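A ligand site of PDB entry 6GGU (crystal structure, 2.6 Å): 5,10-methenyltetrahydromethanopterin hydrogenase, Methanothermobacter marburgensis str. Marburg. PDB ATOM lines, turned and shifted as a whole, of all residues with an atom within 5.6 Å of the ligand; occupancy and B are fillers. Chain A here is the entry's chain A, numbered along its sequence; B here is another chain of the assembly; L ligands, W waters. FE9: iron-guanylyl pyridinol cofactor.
The side-chain carboxylate (OD2) of Asp 189 of chain B binds an iron atom (FE) of the ligand, at 2.3 Å. The backbone NH (N) of Cys 172 is in hydrogen-bond range of an oxygen (O18) of the ligand (3.0 Å). An iron atom (FE) of the ligand is bound by the side-chain sulfur of Cys 172 (2.6 Å). The side-chain carboxylate of Asp 63 is in hydrogen-bond range of an oxygen (O3') of the ligand, at 2.7 Å. An oxygen (O3') of the ligand sits at hydrogen-bond distance from the backbone NH of Gly 9 (2.8 Å). The backbone carbonyl oxygen (O) of Ala 62 is in hydrogen-bond range of a nitrogen (N2A) of the ligand (2.9 Å). The side-chain carboxylate (OD1) of Asp 131 sits at hydrogen-bond distance from a nitrogen (N2A) of the ligand (3.0 Å). The indole nitrogen (NE1) of Trp 144 lies close to an oxygen (O2P) of the ligand (3.4 Å). O2P of the ligand is in hydrogen-bond range of N of Cys 10, at 3.1 Å. The backbone NH (N) of Ala 206 sits at hydrogen-bond distance from an oxygen (O2F) of the ligand (3.3 Å).
OD1 of Asp 189 of chain B is in hydrogen-bond range of OG1 of Thr 192 of chain B (2.7 Å). The backbone NH (N) of Ala 8 is in hydrogen-bond range of the side-chain carboxylate (OD2) of Asp 63 (2.8 Å). The side-chain carboxylate (OD1) of Asp 63 sits at hydrogen-bond distance from the backbone NH (N) of Val 65 (2.9 Å). The backbone carbonyl oxygen of Ala 62 is in hydrogen-bond range of the backbone NH of Gly 7, 2.8 Å away. N of Ala 62 is in hydrogen-bond range of O of Ile 5. The backbone NH (N) of Trp 144 is in hydrogen-bond range of the backbone carbonyl oxygen (O) of Leu 6 (2.9 Å). OG1 of Thr 173 lies within hydrogen-bond range of O of Phe 145. The backbone NH (N) of Gly 205 is in hydrogen-bond range of a ring nitrogen (ND1) of His 203 (2.9 Å).
The backbone NH (N) of Gly 7 sits close to a nitrogen (N2A) of the ligand. Leu 6 touches the ligand. Ala 8 touches the ligand (N to O3', 3.8 Å). OG1 of Thr 13 touches C3M of the ligand, 3.3 Å away. Pro 64 touches the ligand. Pro 110 touches the ligand (CB to O2', 3.1 Å). Pro 111 touches the ligand. Phe 145 touches the ligand. CG of Pro 146 touches C8A of the ligand (3.5 Å). Ile 154 touches the ligand. Ala 171 touches the ligand. Thr 173 touches the ligand. His 203 touches the ligand. Pro 204 touches the ligand. Gly 205 touches the ligand. CA of Val 207 touches O1F of the ligand (3.6 Å). Pro 208 touches the ligand. Val 191 of chain B touches the ligand. Hydrophobic or aromatic side chains within 4 Å of the ligand: Leu 6, Pro 64, Pro 110, Pro 111, Trp 144, Phe 145, Pro 146, Ile 154, Ala 171, His 203, Pro 204, Val 207, Pro 208 and Val 191 of chain B. The nearest printed residue that does not touch the ligand is His 14 (4.04 Å).
Water W2 lies within hydrogen-bond range of an oxygen (O2P) of the ligand (2.5 Å), the side-chain hydroxyl (OG) of Ser 42 (2.7 Å), a ring nitrogen (NE2) of His 14 (2.8 Å) and the indole nitrogen (NE1) of Trp 144 (3.3 Å). Water W3 lies within hydrogen-bond range of O1P of the ligand, OG1 of Thr 13 and O of Cys 10. Water W1 lies within hydrogen-bond range of an oxygen (O2F) of the ligand (3.2 Å) and the backbone carbonyl oxygen of Gly 188 of chain B (3.3 Å).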
ATOM      1  N   ILE A   5      10.996 -25.622   7.616  1.00  0.00           N
ATOM      2  CA  ILE A   5      10.858 -24.614   6.573  1.00  0.00           C
ATOM      3  C   ILE A   5       9.559 -24.883   5.852  1.00  0.00           C
ATOM      4  O   ILE A   5       9.338 -25.996   5.409  1.00  0.00           O
ATOM      5  CB  ILE A   5      12.020 -24.650   5.566  1.00  0.00           C
ATOM      6  CG1 ILE A   5      13.292 -24.126   6.235  1.00  0.00           C
ATOM      7  CG2 ILE A   5      11.655 -23.852   4.279  1.00  0.00           C
ATOM      8  CD1 ILE A   5      14.446 -24.536   5.575  1.00  0.00           C
ATOM      9  N   LEU A   6       8.689 -23.881   5.753  1.00  0.00           N
ATOM     10  CA  LEU A   6       7.412 -24.009   5.063  1.00  0.00           C
ATOM     11  C   LEU A   6       7.517 -23.114   3.825  1.00  0.00           C
ATOM     12  O   LEU A   6       7.363 -21.906   3.914  1.00  0.00           O
ATOM     13  CB  LEU A   6       6.269 -23.583   5.965  1.00  0.00           C
ATOM     14  CG  LEU A   6       5.768 -24.616   6.966  1.00  0.00           C
ATOM     15  CD1 LEU A   6       6.844 -25.027   7.918  1.00  0.00           C
ATOM     16  CD2 LEU A   6       4.548 -24.106   7.768  1.00  0.00           C
ATOM     17  N   GLY A   7       7.817 -23.726   2.686  1.00  0.00           N
ATOM     18  CA  GLY A   7       7.982 -23.026   1.417  1.00  0.00           C
ATOM     19  C   GLY A   7       9.415 -23.144   0.935  1.00  0.00           C
ATOM     20  O   GLY A   7      10.337 -22.627   1.576  1.00  0.00           O
ATOM     21  N   ALA A   8       9.614 -23.855  -0.191  1.00  0.00           N
ATOM     22  CA  ALA A   8      10.940 -24.041  -0.780  1.00  0.00           C
ATOM     23  C   ALA A   8      11.271 -22.827  -1.634  1.00  0.00           C
ATOM     24  O   ALA A   8      12.432 -22.433  -1.745  1.00  0.00           O
ATOM     25  CB  ALA A   8      10.948 -25.304  -1.645  1.00  0.00           C
ATOM     26  N   GLY A   9      10.230 -22.243  -2.238  1.00  0.00           N
ATOM     27  CA  GLY A   9      10.353 -21.066  -3.085  1.00  0.00           C
ATOM     28  C   GLY A   9      10.675 -21.421  -4.512  1.00  0.00           C
ATOM     29  O   GLY A   9      10.812 -22.592  -4.831  1.00  0.00           O
ATOM     30  N   CYS A  10      10.780 -20.421  -5.389  1.00  0.00           N
ATOM     31  CA  CYS A  10      11.094 -20.633  -6.796  1.00  0.00           C
ATOM     32  C   CYS A  10      12.091 -19.599  -7.286  1.00  0.00           C
ATOM     33  O   CYS A  10      12.003 -18.431  -6.916  1.00  0.00           O
ATOM     34  CB  CYS A  10       9.829 -20.640  -7.649  1.00  0.00           C
ATOM     35  SG  CYS A  10      10.142 -20.756  -9.426  1.00  0.00           S
ATOM     36  N   THR A  13      11.592 -15.780 -10.536  1.00  0.00           N
ATOM     37  CA  THR A  13      11.609 -14.337 -10.289  1.00  0.00           C
ATOM     38  C   THR A  13      13.020 -13.829 -10.076  1.00  0.00           C
ATOM     39  O   THR A  13      13.286 -12.679 -10.423  1.00  0.00           O
ATOM     40  CB  THR A  13      10.725 -14.020  -9.085  1.00  0.00           C
ATOM     41  OG1 THR A  13      11.080 -14.869  -7.999  1.00  0.00           O
ATOM     42  CG2 THR A  13       9.258 -14.170  -9.398  1.00  0.00           C
ATOM     43  N   HIS A  14      13.927 -14.662  -9.514  1.00  0.00           N
ATOM     44  CA  HIS A  14      15.307 -14.228  -9.280  1.00  0.00           C
ATOM     45  C   HIS A  14      16.002 -14.102 -10.639  1.00  0.00           C
ATOM     46  O   HIS A  14      16.631 -13.081 -10.926  1.00  0.00           O
ATOM     47  CB  HIS A  14      16.090 -15.204  -8.379  1.00  0.00           C
ATOM     48  CG  HIS A  14      15.399 -15.588  -7.102  1.00  0.00           C
ATOM     49  ND1 HIS A  14      16.035 -16.355  -6.139  1.00  0.00           N
ATOM     50  CD2 HIS A  14      14.157 -15.290  -6.669  1.00  0.00           C
ATOM     51  CE1 HIS A  14      15.162 -16.491  -5.153  1.00  0.00           C
ATOM     52  NE2 HIS A  14      14.009 -15.888  -5.446  1.00  0.00           N
ATOM     53  N   SER A  42      16.873 -19.409  -2.135  1.00  0.00           N
ATOM     54  CA  SER A  42      15.824 -19.131  -1.172  1.00  0.00           C
ATOM     55  C   SER A  42      16.036 -19.845   0.174  1.00  0.00           C
ATOM     56  O   SER A  42      17.166 -19.846   0.673  1.00  0.00           O
ATOM     57  CB  SER A  42      14.458 -19.431  -1.785  1.00  0.00           C
ATOM     58  OG  SER A  42      14.280 -18.617  -2.924  1.00  0.00           O
ATOM     59  N   ALA A  62       8.860 -28.159   3.951  1.00  0.00           N
ATOM     60  CA  ALA A  62       7.482 -28.494   3.598  1.00  0.00           C
ATOM     61  C   ALA A  62       6.974 -27.613   2.457  1.00  0.00           C
ATOM     62  O   ALA A  62       7.056 -26.391   2.547  1.00  0.00           O
ATOM     63  CB  ALA A  62       6.583 -28.325   4.803  1.00  0.00           C
ATOM     64  N   ASP A  63       6.468 -28.237   1.387  1.00  0.00           N
ATOM     65  CA  ASP A  63       5.962 -27.470   0.261  1.00  0.00           C
ATOM     66  C   ASP A  63       5.063 -28.321  -0.630  1.00  0.00           C
ATOM     67  O   ASP A  63       5.512 -29.346  -1.138  1.00  0.00           O
ATOM     68  CB  ASP A  63       7.122 -26.896  -0.585  1.00  0.00           C
ATOM     69  CG  ASP A  63       6.707 -25.776  -1.523  1.00  0.00           C
ATOM     70  OD1 ASP A  63       5.639 -25.903  -2.154  1.00  0.00           O
ATOM     71  OD2 ASP A  63       7.456 -24.792  -1.622  1.00  0.00           O
ATOM     72  N   PRO A  64       3.818 -27.896  -0.875  1.00  0.00           N
ATOM     73  CA  PRO A  64       2.934 -28.676  -1.753  1.00  0.00           C
ATOM     74  C   PRO A  64       3.575 -28.985  -3.124  1.00  0.00           C
ATOM     75  O   PRO A  64       3.263 -30.019  -3.716  1.00  0.00           O
ATOM     76  CB  PRO A  64       1.690 -27.776  -1.890  1.00  0.00           C
ATOM     77  CG  PRO A  64       2.109 -26.458  -1.416  1.00  0.00           C
ATOM     78  CD  PRO A  64       3.119 -26.700  -0.381  1.00  0.00           C
ATOM     79  N   VAL A  65       4.469 -28.104  -3.608  1.00  0.00           N
ATOM     80  CA  VAL A  65       5.154 -28.280  -4.901  1.00  0.00           C
ATOM     81  C   VAL A  65       5.862 -29.624  -5.063  1.00  0.00           C
ATOM     82  O   VAL A  65       5.919 -30.130  -6.185  1.00  0.00           O
ATOM     83  CB  VAL A  65       6.135 -27.108  -5.210  1.00  0.00           C
ATOM     84  CG1 VAL A  65       7.436 -27.288  -4.435  1.00  0.00           C
ATOM     85  CG2 VAL A  65       6.403 -27.040  -6.707  1.00  0.00           C
ATOM     86  N   PRO A 110       4.287 -21.240  -8.483  1.00  0.00           N
ATOM     87  CA  PRO A 110       4.098 -22.043  -7.270  1.00  0.00           C
ATOM     88  C   PRO A 110       2.680 -21.900  -6.713  1.00  0.00           C
ATOM     89  O   PRO A 110       2.038 -20.873  -6.957  1.00  0.00           O
ATOM     90  CB  PRO A 110       5.173 -21.508  -6.303  1.00  0.00           C
ATOM     91  CG  PRO A 110       6.113 -20.733  -7.147  1.00  0.00           C
ATOM     92  CD  PRO A 110       5.313 -20.198  -8.296  1.00  0.00           C
ATOM     93  N   PRO A 111       2.159 -22.881  -5.969  1.00  0.00           N
ATOM     94  CA  PRO A 111       2.787 -24.161  -5.597  1.00  0.00           C
ATOM     95  C   PRO A 111       2.728 -25.251  -6.666  1.00  0.00           C
ATOM     96  O   PRO A 111       3.089 -26.382  -6.366  1.00  0.00           O
ATOM     97  CB  PRO A 111       1.997 -24.549  -4.336  1.00  0.00           C
ATOM     98  CG  PRO A 111       0.613 -24.053  -4.630  1.00  0.00           C
ATOM     99  CD  PRO A 111       0.797 -22.774  -5.414  1.00  0.00           C
ATOM    100  N   GLU A 112       2.296 -24.950  -7.907  1.00  0.00           N
ATOM    101  CA  GLU A 112       2.206 -25.979  -8.945  1.00  0.00           C
ATOM    102  C   GLU A 112       3.569 -26.219  -9.643  1.00  0.00           C
ATOM    103  O   GLU A 112       3.770 -27.275 -10.222  1.00  0.00           O
ATOM    104  CB  GLU A 112       1.125 -25.638  -9.981  1.00  0.00           C
ATOM    105  CG  GLU A 112      -0.256 -25.386  -9.384  1.00  0.00           C
ATOM    106  CD  GLU A 112      -0.941 -26.578  -8.759  1.00  0.00           C
ATOM    107  OE1 GLU A 112      -1.009 -26.639  -7.510  1.00  0.00           O
ATOM    108  OE2 GLU A 112      -1.438 -27.451  -9.526  1.00  0.00           O
ATOM    109  N   GLY A 113       4.464 -25.238  -9.586  1.00  0.00           N
ATOM    110  CA  GLY A 113       5.790 -25.369 -10.191  1.00  0.00           C
ATOM    111  C   GLY A 113       6.863 -24.615  -9.431  1.00  0.00           C
ATOM    112  O   GLY A 113       6.580 -23.593  -8.817  1.00  0.00           O
ATOM    113  N   ALA A 114       8.108 -25.125  -9.455  1.00  0.00           N
ATOM    114  CA  ALA A 114       9.220 -24.474  -8.760  1.00  0.00           C
ATOM    115  C   ALA A 114      10.519 -24.759  -9.453  1.00  0.00           C
ATOM    116  O   ALA A 114      10.791 -25.917  -9.770  1.00  0.00           O
ATOM    117  CB  ALA A 114       9.298 -24.948  -7.325  1.00  0.00           C
ATOM    118  N   ASP A 131       2.333 -29.479   5.818  1.00  0.00           N
ATOM    119  CA  ASP A 131       2.901 -28.561   6.813  1.00  0.00           C
ATOM    120  C   ASP A 131       2.730 -29.003   8.271  1.00  0.00           C
ATOM    121  O   ASP A 131       3.613 -28.742   9.079  1.00  0.00           O
ATOM    122  CB  ASP A 131       2.251 -27.170   6.673  1.00  0.00           C
ATOM    123  CG  ASP A 131       2.223 -26.611   5.255  1.00  0.00           C
ATOM    124  OD1 ASP A 131       3.187 -26.857   4.504  1.00  0.00           O
ATOM    125  OD2 ASP A 131       1.225 -25.939   4.898  1.00  0.00           O
ATOM    126  N   TRP A 144       8.022 -19.066   4.331  1.00  0.00           N
ATOM    127  CA  TRP A 144       8.425 -18.477   3.057  1.00  0.00           C
ATOM    128  C   TRP A 144       7.171 -18.609   2.193  1.00  0.00           C
ATOM    129  O   TRP A 144       7.168 -19.321   1.176  1.00  0.00           O
ATOM    130  CB  TRP A 144       9.574 -19.305   2.463  1.00  0.00           C
ATOM    131  CG  TRP A 144      10.307 -18.685   1.310  1.00  0.00           C
ATOM    132  CD1 TRP A 144      10.212 -19.014  -0.008  1.00  0.00           C
ATOM    133  CD2 TRP A 144      11.330 -17.692   1.398  1.00  0.00           C
ATOM    134  NE1 TRP A 144      11.078 -18.251  -0.755  1.00  0.00           N
ATOM    135  CE2 TRP A 144      11.787 -17.446   0.089  1.00  0.00           C
ATOM    136  CE3 TRP A 144      11.912 -16.983   2.470  1.00  0.00           C
ATOM    137  CZ2 TRP A 144      12.793 -16.505  -0.191  1.00  0.00           C
ATOM    138  CZ3 TRP A 144      12.918 -16.065   2.188  1.00  0.00           C
ATOM    139  CH2 TRP A 144      13.352 -15.845   0.875  1.00  0.00           C
ATOM    140  N   PHE A 145       6.083 -17.952   2.627  1.00  0.00           N
ATOM    141  CA  PHE A 145       4.808 -18.050   1.902  1.00  0.00           C
ATOM    142  C   PHE A 145       4.611 -17.024   0.810  1.00  0.00           C
ATOM    143  O   PHE A 145       5.308 -16.024   0.789  1.00  0.00           O
ATOM    144  CB  PHE A 145       3.644 -18.000   2.907  1.00  0.00           C
ATOM    145  CG  PHE A 145       3.627 -19.142   3.877  1.00  0.00           C
ATOM    146  CD1 PHE A 145       3.950 -20.427   3.474  1.00  0.00           C
ATOM    147  CD2 PHE A 145       3.283 -18.936   5.204  1.00  0.00           C
ATOM    148  CE1 PHE A 145       3.928 -21.483   4.374  1.00  0.00           C
ATOM    149  CE2 PHE A 145       3.245 -19.995   6.097  1.00  0.00           C
ATOM    150  CZ  PHE A 145       3.571 -21.262   5.678  1.00  0.00           C
ATOM    151  N   PRO A 146       3.633 -17.246  -0.092  1.00  0.00           N
ATOM    152  CA  PRO A 146       3.398 -16.263  -1.152  1.00  0.00           C
ATOM    153  C   PRO A 146       2.743 -14.989  -0.630  1.00  0.00           C
ATOM    154  O   PRO A 146       2.080 -15.003   0.404  1.00  0.00           O
ATOM    155  CB  PRO A 146       2.420 -16.984  -2.099  1.00  0.00           C
ATOM    156  CG  PRO A 146       2.382 -18.402  -1.658  1.00  0.00           C
ATOM    157  CD  PRO A 146       2.703 -18.383  -0.209  1.00  0.00           C
ATOM    158  N   ILE A 154      -3.175 -20.569   4.950  1.00  0.00           N
ATOM    159  CA  ILE A 154      -2.077 -21.534   4.885  1.00  0.00           C
ATOM    160  C   ILE A 154      -1.674 -21.847   6.331  1.00  0.00           C
ATOM    161  O   ILE A 154      -1.502 -23.007   6.700  1.00  0.00           O
ATOM    162  CB  ILE A 154      -0.864 -20.968   4.096  1.00  0.00           C
ATOM    163  CG1 ILE A 154      -1.177 -20.807   2.591  1.00  0.00           C
ATOM    164  CG2 ILE A 154       0.391 -21.815   4.302  1.00  0.00           C
ATOM    165  CD1 ILE A 154      -0.099 -19.932   1.806  1.00  0.00           C
ATOM    166  N   LYS A 157      -4.033 -24.091   9.025  1.00  0.00           N
ATOM    167  CA  LYS A 157      -3.979 -25.555   8.937  1.00  0.00           C
ATOM    168  C   LYS A 157      -2.973 -26.226   9.885  1.00  0.00           C
ATOM    169  O   LYS A 157      -3.183 -27.388  10.208  1.00  0.00           O
ATOM    170  CB  LYS A 157      -3.647 -26.001   7.522  1.00  0.00           C
ATOM    171  CG  LYS A 157      -4.749 -25.735   6.527  1.00  0.00           C
ATOM    172  CD  LYS A 157      -4.416 -26.417   5.203  1.00  0.00           C
ATOM    173  CE  LYS A 157      -4.433 -25.486   4.016  1.00  0.00           C
ATOM    174  NZ  LYS A 157      -5.781 -25.418   3.403  1.00  0.00           N
ATOM    175  N   ALA A 171       9.146 -13.600   6.021  1.00  0.00           N
ATOM    176  CA  ALA A 171      10.124 -12.970   5.152  1.00  0.00           C
ATOM    177  C   ALA A 171       9.477 -11.794   4.403  1.00  0.00           C
ATOM    178  O   ALA A 171       8.435 -11.316   4.824  1.00  0.00           O
ATOM    179  CB  ALA A 171      10.682 -14.008   4.194  1.00  0.00           C
ATOM    180  N   CYS A 172      10.082 -11.330   3.293  1.00  0.00           N
ATOM    181  CA  CYS A 172       9.632 -10.149   2.534  1.00  0.00           C
ATOM    182  C   CYS A 172       8.192 -10.139   2.024  1.00  0.00           C
ATOM    183  O   CYS A 172       7.709  -9.058   1.677  1.00  0.00           O
ATOM    184  CB  CYS A 172      10.598  -9.878   1.390  1.00  0.00           C
ATOM    185  SG  CYS A 172      10.127 -10.670  -0.154  1.00  0.00           S
ATOM    186  N   THR A 173       7.511 -11.279   1.955  1.00  0.00           N
ATOM    187  CA  THR A 173       6.132 -11.365   1.466  1.00  0.00           C
ATOM    188  C   THR A 173       5.064 -10.831   2.414  1.00  0.00           C
ATOM    189  O   THR A 173       3.925 -10.664   1.979  1.00  0.00           O
ATOM    190  CB  THR A 173       5.811 -12.827   1.107  1.00  0.00           C
ATOM    191  OG1 THR A 173       6.135 -13.683   2.218  1.00  0.00           O
ATOM    192  CG2 THR A 173       6.533 -13.270  -0.160  1.00  0.00           C
ATOM    193  N   HIS A 203      14.241 -12.316   7.647  1.00  0.00           N
ATOM    194  CA  HIS A 203      14.163 -11.577   6.390  1.00  0.00           C
ATOM    195  C   HIS A 203      15.531 -11.402   5.718  1.00  0.00           C
ATOM    196  O   HIS A 203      16.392 -10.687   6.235  1.00  0.00           O
ATOM    197  CB  HIS A 203      13.474 -10.223   6.654  1.00  0.00           C
ATOM    198  CG  HIS A 203      13.030  -9.540   5.400  1.00  0.00           C
ATOM    199  ND1 HIS A 203      13.752  -9.641   4.230  1.00  0.00           N
ATOM    200  CD2 HIS A 203      11.929  -8.767   5.179  1.00  0.00           C
ATOM    201  CE1 HIS A 203      13.081  -8.955   3.324  1.00  0.00           C
ATOM    202  NE2 HIS A 203      11.985  -8.390   3.845  1.00  0.00           N
ATOM    203  N   PRO A 204      15.769 -12.026   4.564  1.00  0.00           N
ATOM    204  CA  PRO A 204      17.098 -11.882   3.944  1.00  0.00           C
ATOM    205  C   PRO A 204      17.474 -10.495   3.458  1.00  0.00           C
ATOM    206  O   PRO A 204      18.664 -10.191   3.351  1.00  0.00           O
ATOM    207  CB  PRO A 204      17.068 -12.916   2.804  1.00  0.00           C
ATOM    208  CG  PRO A 204      15.622 -13.079   2.485  1.00  0.00           C
ATOM    209  CD  PRO A 204      14.907 -12.935   3.785  1.00  0.00           C
ATOM    210  N   GLY A 205      16.484  -9.678   3.129  1.00  0.00           N
ATOM    211  CA  GLY A 205      16.754  -8.340   2.628  1.00  0.00           C
ATOM    212  C   GLY A 205      17.439  -8.403   1.279  1.00  0.00           C
ATOM    213  O   GLY A 205      18.123  -7.458   0.872  1.00  0.00           O
ATOM    214  N   ALA A 206      17.290  -9.556   0.599  1.00  0.00           N
ATOM    215  CA  ALA A 206      17.848  -9.865  -0.714  1.00  0.00           C
ATOM    216  C   ALA A 206      17.560 -11.313  -0.964  1.00  0.00           C
ATOM    217  O   ALA A 206      16.959 -11.966  -0.128  1.00  0.00           O
ATOM    218  CB  ALA A 206      19.357  -9.650  -0.710  1.00  0.00           C
ATOM    219  N   VAL A 207      17.990 -11.847  -2.108  1.00  0.00           N
ATOM    220  CA  VAL A 207      17.803 -13.262  -2.377  1.00  0.00           C
ATOM    221  C   VAL A 207      18.820 -13.977  -1.479  1.00  0.00           C
ATOM    222  O   VAL A 207      20.008 -13.672  -1.545  1.00  0.00           O
ATOM    223  CB  VAL A 207      17.950 -13.604  -3.860  1.00  0.00           C
ATOM    224  CG1 VAL A 207      16.858 -12.954  -4.669  1.00  0.00           C
ATOM    225  CG2 VAL A 207      19.334 -13.227  -4.418  1.00  0.00           C
ATOM    226  N   PRO A 208      18.407 -14.903  -0.584  1.00  0.00           N
ATOM    227  CA  PRO A 208      19.376 -15.539   0.314  1.00  0.00           C
ATOM    228  C   PRO A 208      20.676 -16.072  -0.309  1.00  0.00           C
ATOM    229  O   PRO A 208      21.729 -15.981   0.332  1.00  0.00           O
ATOM    230  CB  PRO A 208      18.571 -16.653   0.976  1.00  0.00           C
ATOM    231  CG  PRO A 208      17.169 -16.196   0.930  1.00  0.00           C
ATOM    232  CD  PRO A 208      17.028 -15.369  -0.312  1.00  0.00           C
ATOM    233  N   GLY B 188       8.370  -5.740  -0.596  1.00  0.00           N
ATOM    234  CA  GLY B 188       8.986  -6.582  -1.598  1.00  0.00           C
ATOM    235  C   GLY B 188      10.485  -6.712  -1.424  1.00  0.00           C
ATOM    236  O   GLY B 188      11.006  -6.697  -0.310  1.00  0.00           O
ATOM    237  N   ASP B 189      11.160  -6.856  -2.558  1.00  0.00           N
ATOM    238  CA  ASP B 189      12.605  -7.019  -2.602  1.00  0.00           C
ATOM    239  C   ASP B 189      13.070  -6.613  -3.992  1.00  0.00           C
ATOM    240  O   ASP B 189      12.228  -6.322  -4.847  1.00  0.00           O
ATOM    241  CB  ASP B 189      12.974  -8.483  -2.292  1.00  0.00           C
ATOM    242  CG  ASP B 189      12.211  -9.533  -3.088  1.00  0.00           C
ATOM    243  OD1 ASP B 189      11.398  -9.155  -3.966  1.00  0.00           O
ATOM    244  OD2 ASP B 189      12.406 -10.731  -2.809  1.00  0.00           O
ATOM    245  N   VAL B 191      14.057  -8.359  -6.329  1.00  0.00           N
ATOM    246  CA  VAL B 191      13.481  -9.312  -7.278  1.00  0.00           C
ATOM    247  C   VAL B 191      12.074  -8.920  -7.735  1.00  0.00           C
ATOM    248  O   VAL B 191      11.782  -9.001  -8.912  1.00  0.00           O
ATOM    249  CB  VAL B 191      13.522 -10.728  -6.681  1.00  0.00           C
ATOM    250  CG1 VAL B 191      12.516 -11.642  -7.346  1.00  0.00           C
ATOM    251  CG2 VAL B 191      14.917 -11.307  -6.793  1.00  0.00           C
ATOM    252  N   THR B 192      11.207  -8.518  -6.800  1.00  0.00           N
ATOM    253  CA  THR B 192       9.833  -8.136  -7.149  1.00  0.00           C
ATOM    254  C   THR B 192       9.843  -6.726  -7.712  1.00  0.00           C
ATOM    255  O   THR B 192      10.073  -5.772  -6.958  1.00  0.00           O
ATOM    256  CB  THR B 192       8.912  -8.229  -5.923  1.00  0.00           C
ATOM    257  OG1 THR B 192       9.058  -9.528  -5.330  1.00  0.00           O
ATOM    258  CG2 THR B 192       7.447  -7.979  -6.285  1.00  0.00           C
HETATM  259  O2  FE9 L   1      11.363 -12.783  -3.888  1.00  0.00           O
HETATM  260 FE   FE9 L   1      12.174 -12.127  -0.982  1.00  0.00          FE
HETATM  261  C1F FE9 L   1      13.501 -13.271  -1.541  1.00  0.00           C
HETATM  262  O1F FE9 L   1      14.329 -13.947  -1.914  1.00  0.00           O
HETATM  263  C2F FE9 L   1      13.410 -11.140  -0.101  1.00  0.00           C
HETATM  264  O2F FE9 L   1      14.171 -10.562   0.496  1.00  0.00           O
HETATM  265  C8  FE9 L   1      11.704 -12.975   0.668  1.00  0.00           C
HETATM  266  O18 FE9 L   1      12.297 -12.689   1.702  1.00  0.00           O
HETATM  267  C7  FE9 L   1      10.558 -13.964   0.648  1.00  0.00           C
HETATM  268  C6  FE9 L   1      10.248 -14.207  -0.799  1.00  0.00           C
HETATM  269  N1  FE9 L   1      10.912 -13.384  -1.739  1.00  0.00           N
HETATM  270  C5  FE9 L   1       9.264 -15.229  -1.232  1.00  0.00           C
HETATM  271  C5M FE9 L   1       8.543 -16.084  -0.230  1.00  0.00           C
HETATM  272  C4  FE9 L   1       9.030 -15.376  -2.696  1.00  0.00           C
HETATM  273  C3  FE9 L   1       9.749 -14.498  -3.655  1.00  0.00           C
HETATM  274  C3M FE9 L   1       9.510 -14.648  -5.131  1.00  0.00           C
HETATM  275  C2  FE9 L   1      10.721 -13.506  -3.117  1.00  0.00           C
HETATM  276  O3P FE9 L   1       8.091 -16.230  -3.159  1.00  0.00           O
HETATM  277  P1  FE9 L   1       8.457 -17.688  -3.648  1.00  0.00           P
HETATM  278  O1P FE9 L   1       7.624 -17.924  -4.862  1.00  0.00           O
HETATM  279  O2P FE9 L   1      10.020 -17.790  -3.939  1.00  0.00           O
HETATM  280  O5' FE9 L   1       8.073 -18.721  -2.485  1.00  0.00           O
HETATM  281  C5' FE9 L   1       6.720 -19.042  -2.170  1.00  0.00           C
HETATM  282  C4' FE9 L   1       6.708 -20.513  -1.792  1.00  0.00           C
HETATM  283  O4' FE9 L   1       5.621 -20.821  -0.911  1.00  0.00           O
HETATM  284  C1' FE9 L   1       4.987 -21.989  -1.419  1.00  0.00           C
HETATM  285  C2' FE9 L   1       5.124 -21.862  -2.925  1.00  0.00           C
HETATM  286  O2' FE9 L   1       4.892 -23.081  -3.618  1.00  0.00           O
HETATM  287  C3' FE9 L   1       6.563 -21.382  -3.035  1.00  0.00           C
HETATM  288  O3' FE9 L   1       7.533 -22.449  -3.008  1.00  0.00           O
HETATM  289  N9A FE9 L   1       3.609 -22.215  -0.947  1.00  0.00           N
HETATM  290  C4A FE9 L   1       3.386 -22.975   0.115  1.00  0.00           C
HETATM  291  N3A FE9 L   1       4.205 -23.595   0.986  1.00  0.00           N
HETATM  292  C2A FE9 L   1       3.706 -24.308   2.017  1.00  0.00           C
HETATM  293  N2A FE9 L   1       4.617 -24.882   2.829  1.00  0.00           N
HETATM  294  N1A FE9 L   1       2.380 -24.416   2.250  1.00  0.00           N
HETATM  295  C6A FE9 L   1       1.461 -23.842   1.442  1.00  0.00           C
HETATM  296  O6A FE9 L   1       0.235 -23.970   1.647  1.00  0.00           O
HETATM  297  C5A FE9 L   1       1.938 -23.056   0.287  1.00  0.00           C
HETATM  298  N7A FE9 L   1       1.395 -22.357  -0.719  1.00  0.00           N
HETATM  299  C8A FE9 L   1       2.414 -21.858  -1.475  1.00  0.00           C
HETATM  300  O   HOH W   1      14.037  -7.403   0.815  1.00  0.00           O
HETATM  301  O   HOH W   2      12.328 -16.896  -3.475  1.00  0.00           O
HETATM  302  O   HOH W   3       8.830 -17.128  -7.564  1.00  0.00           O
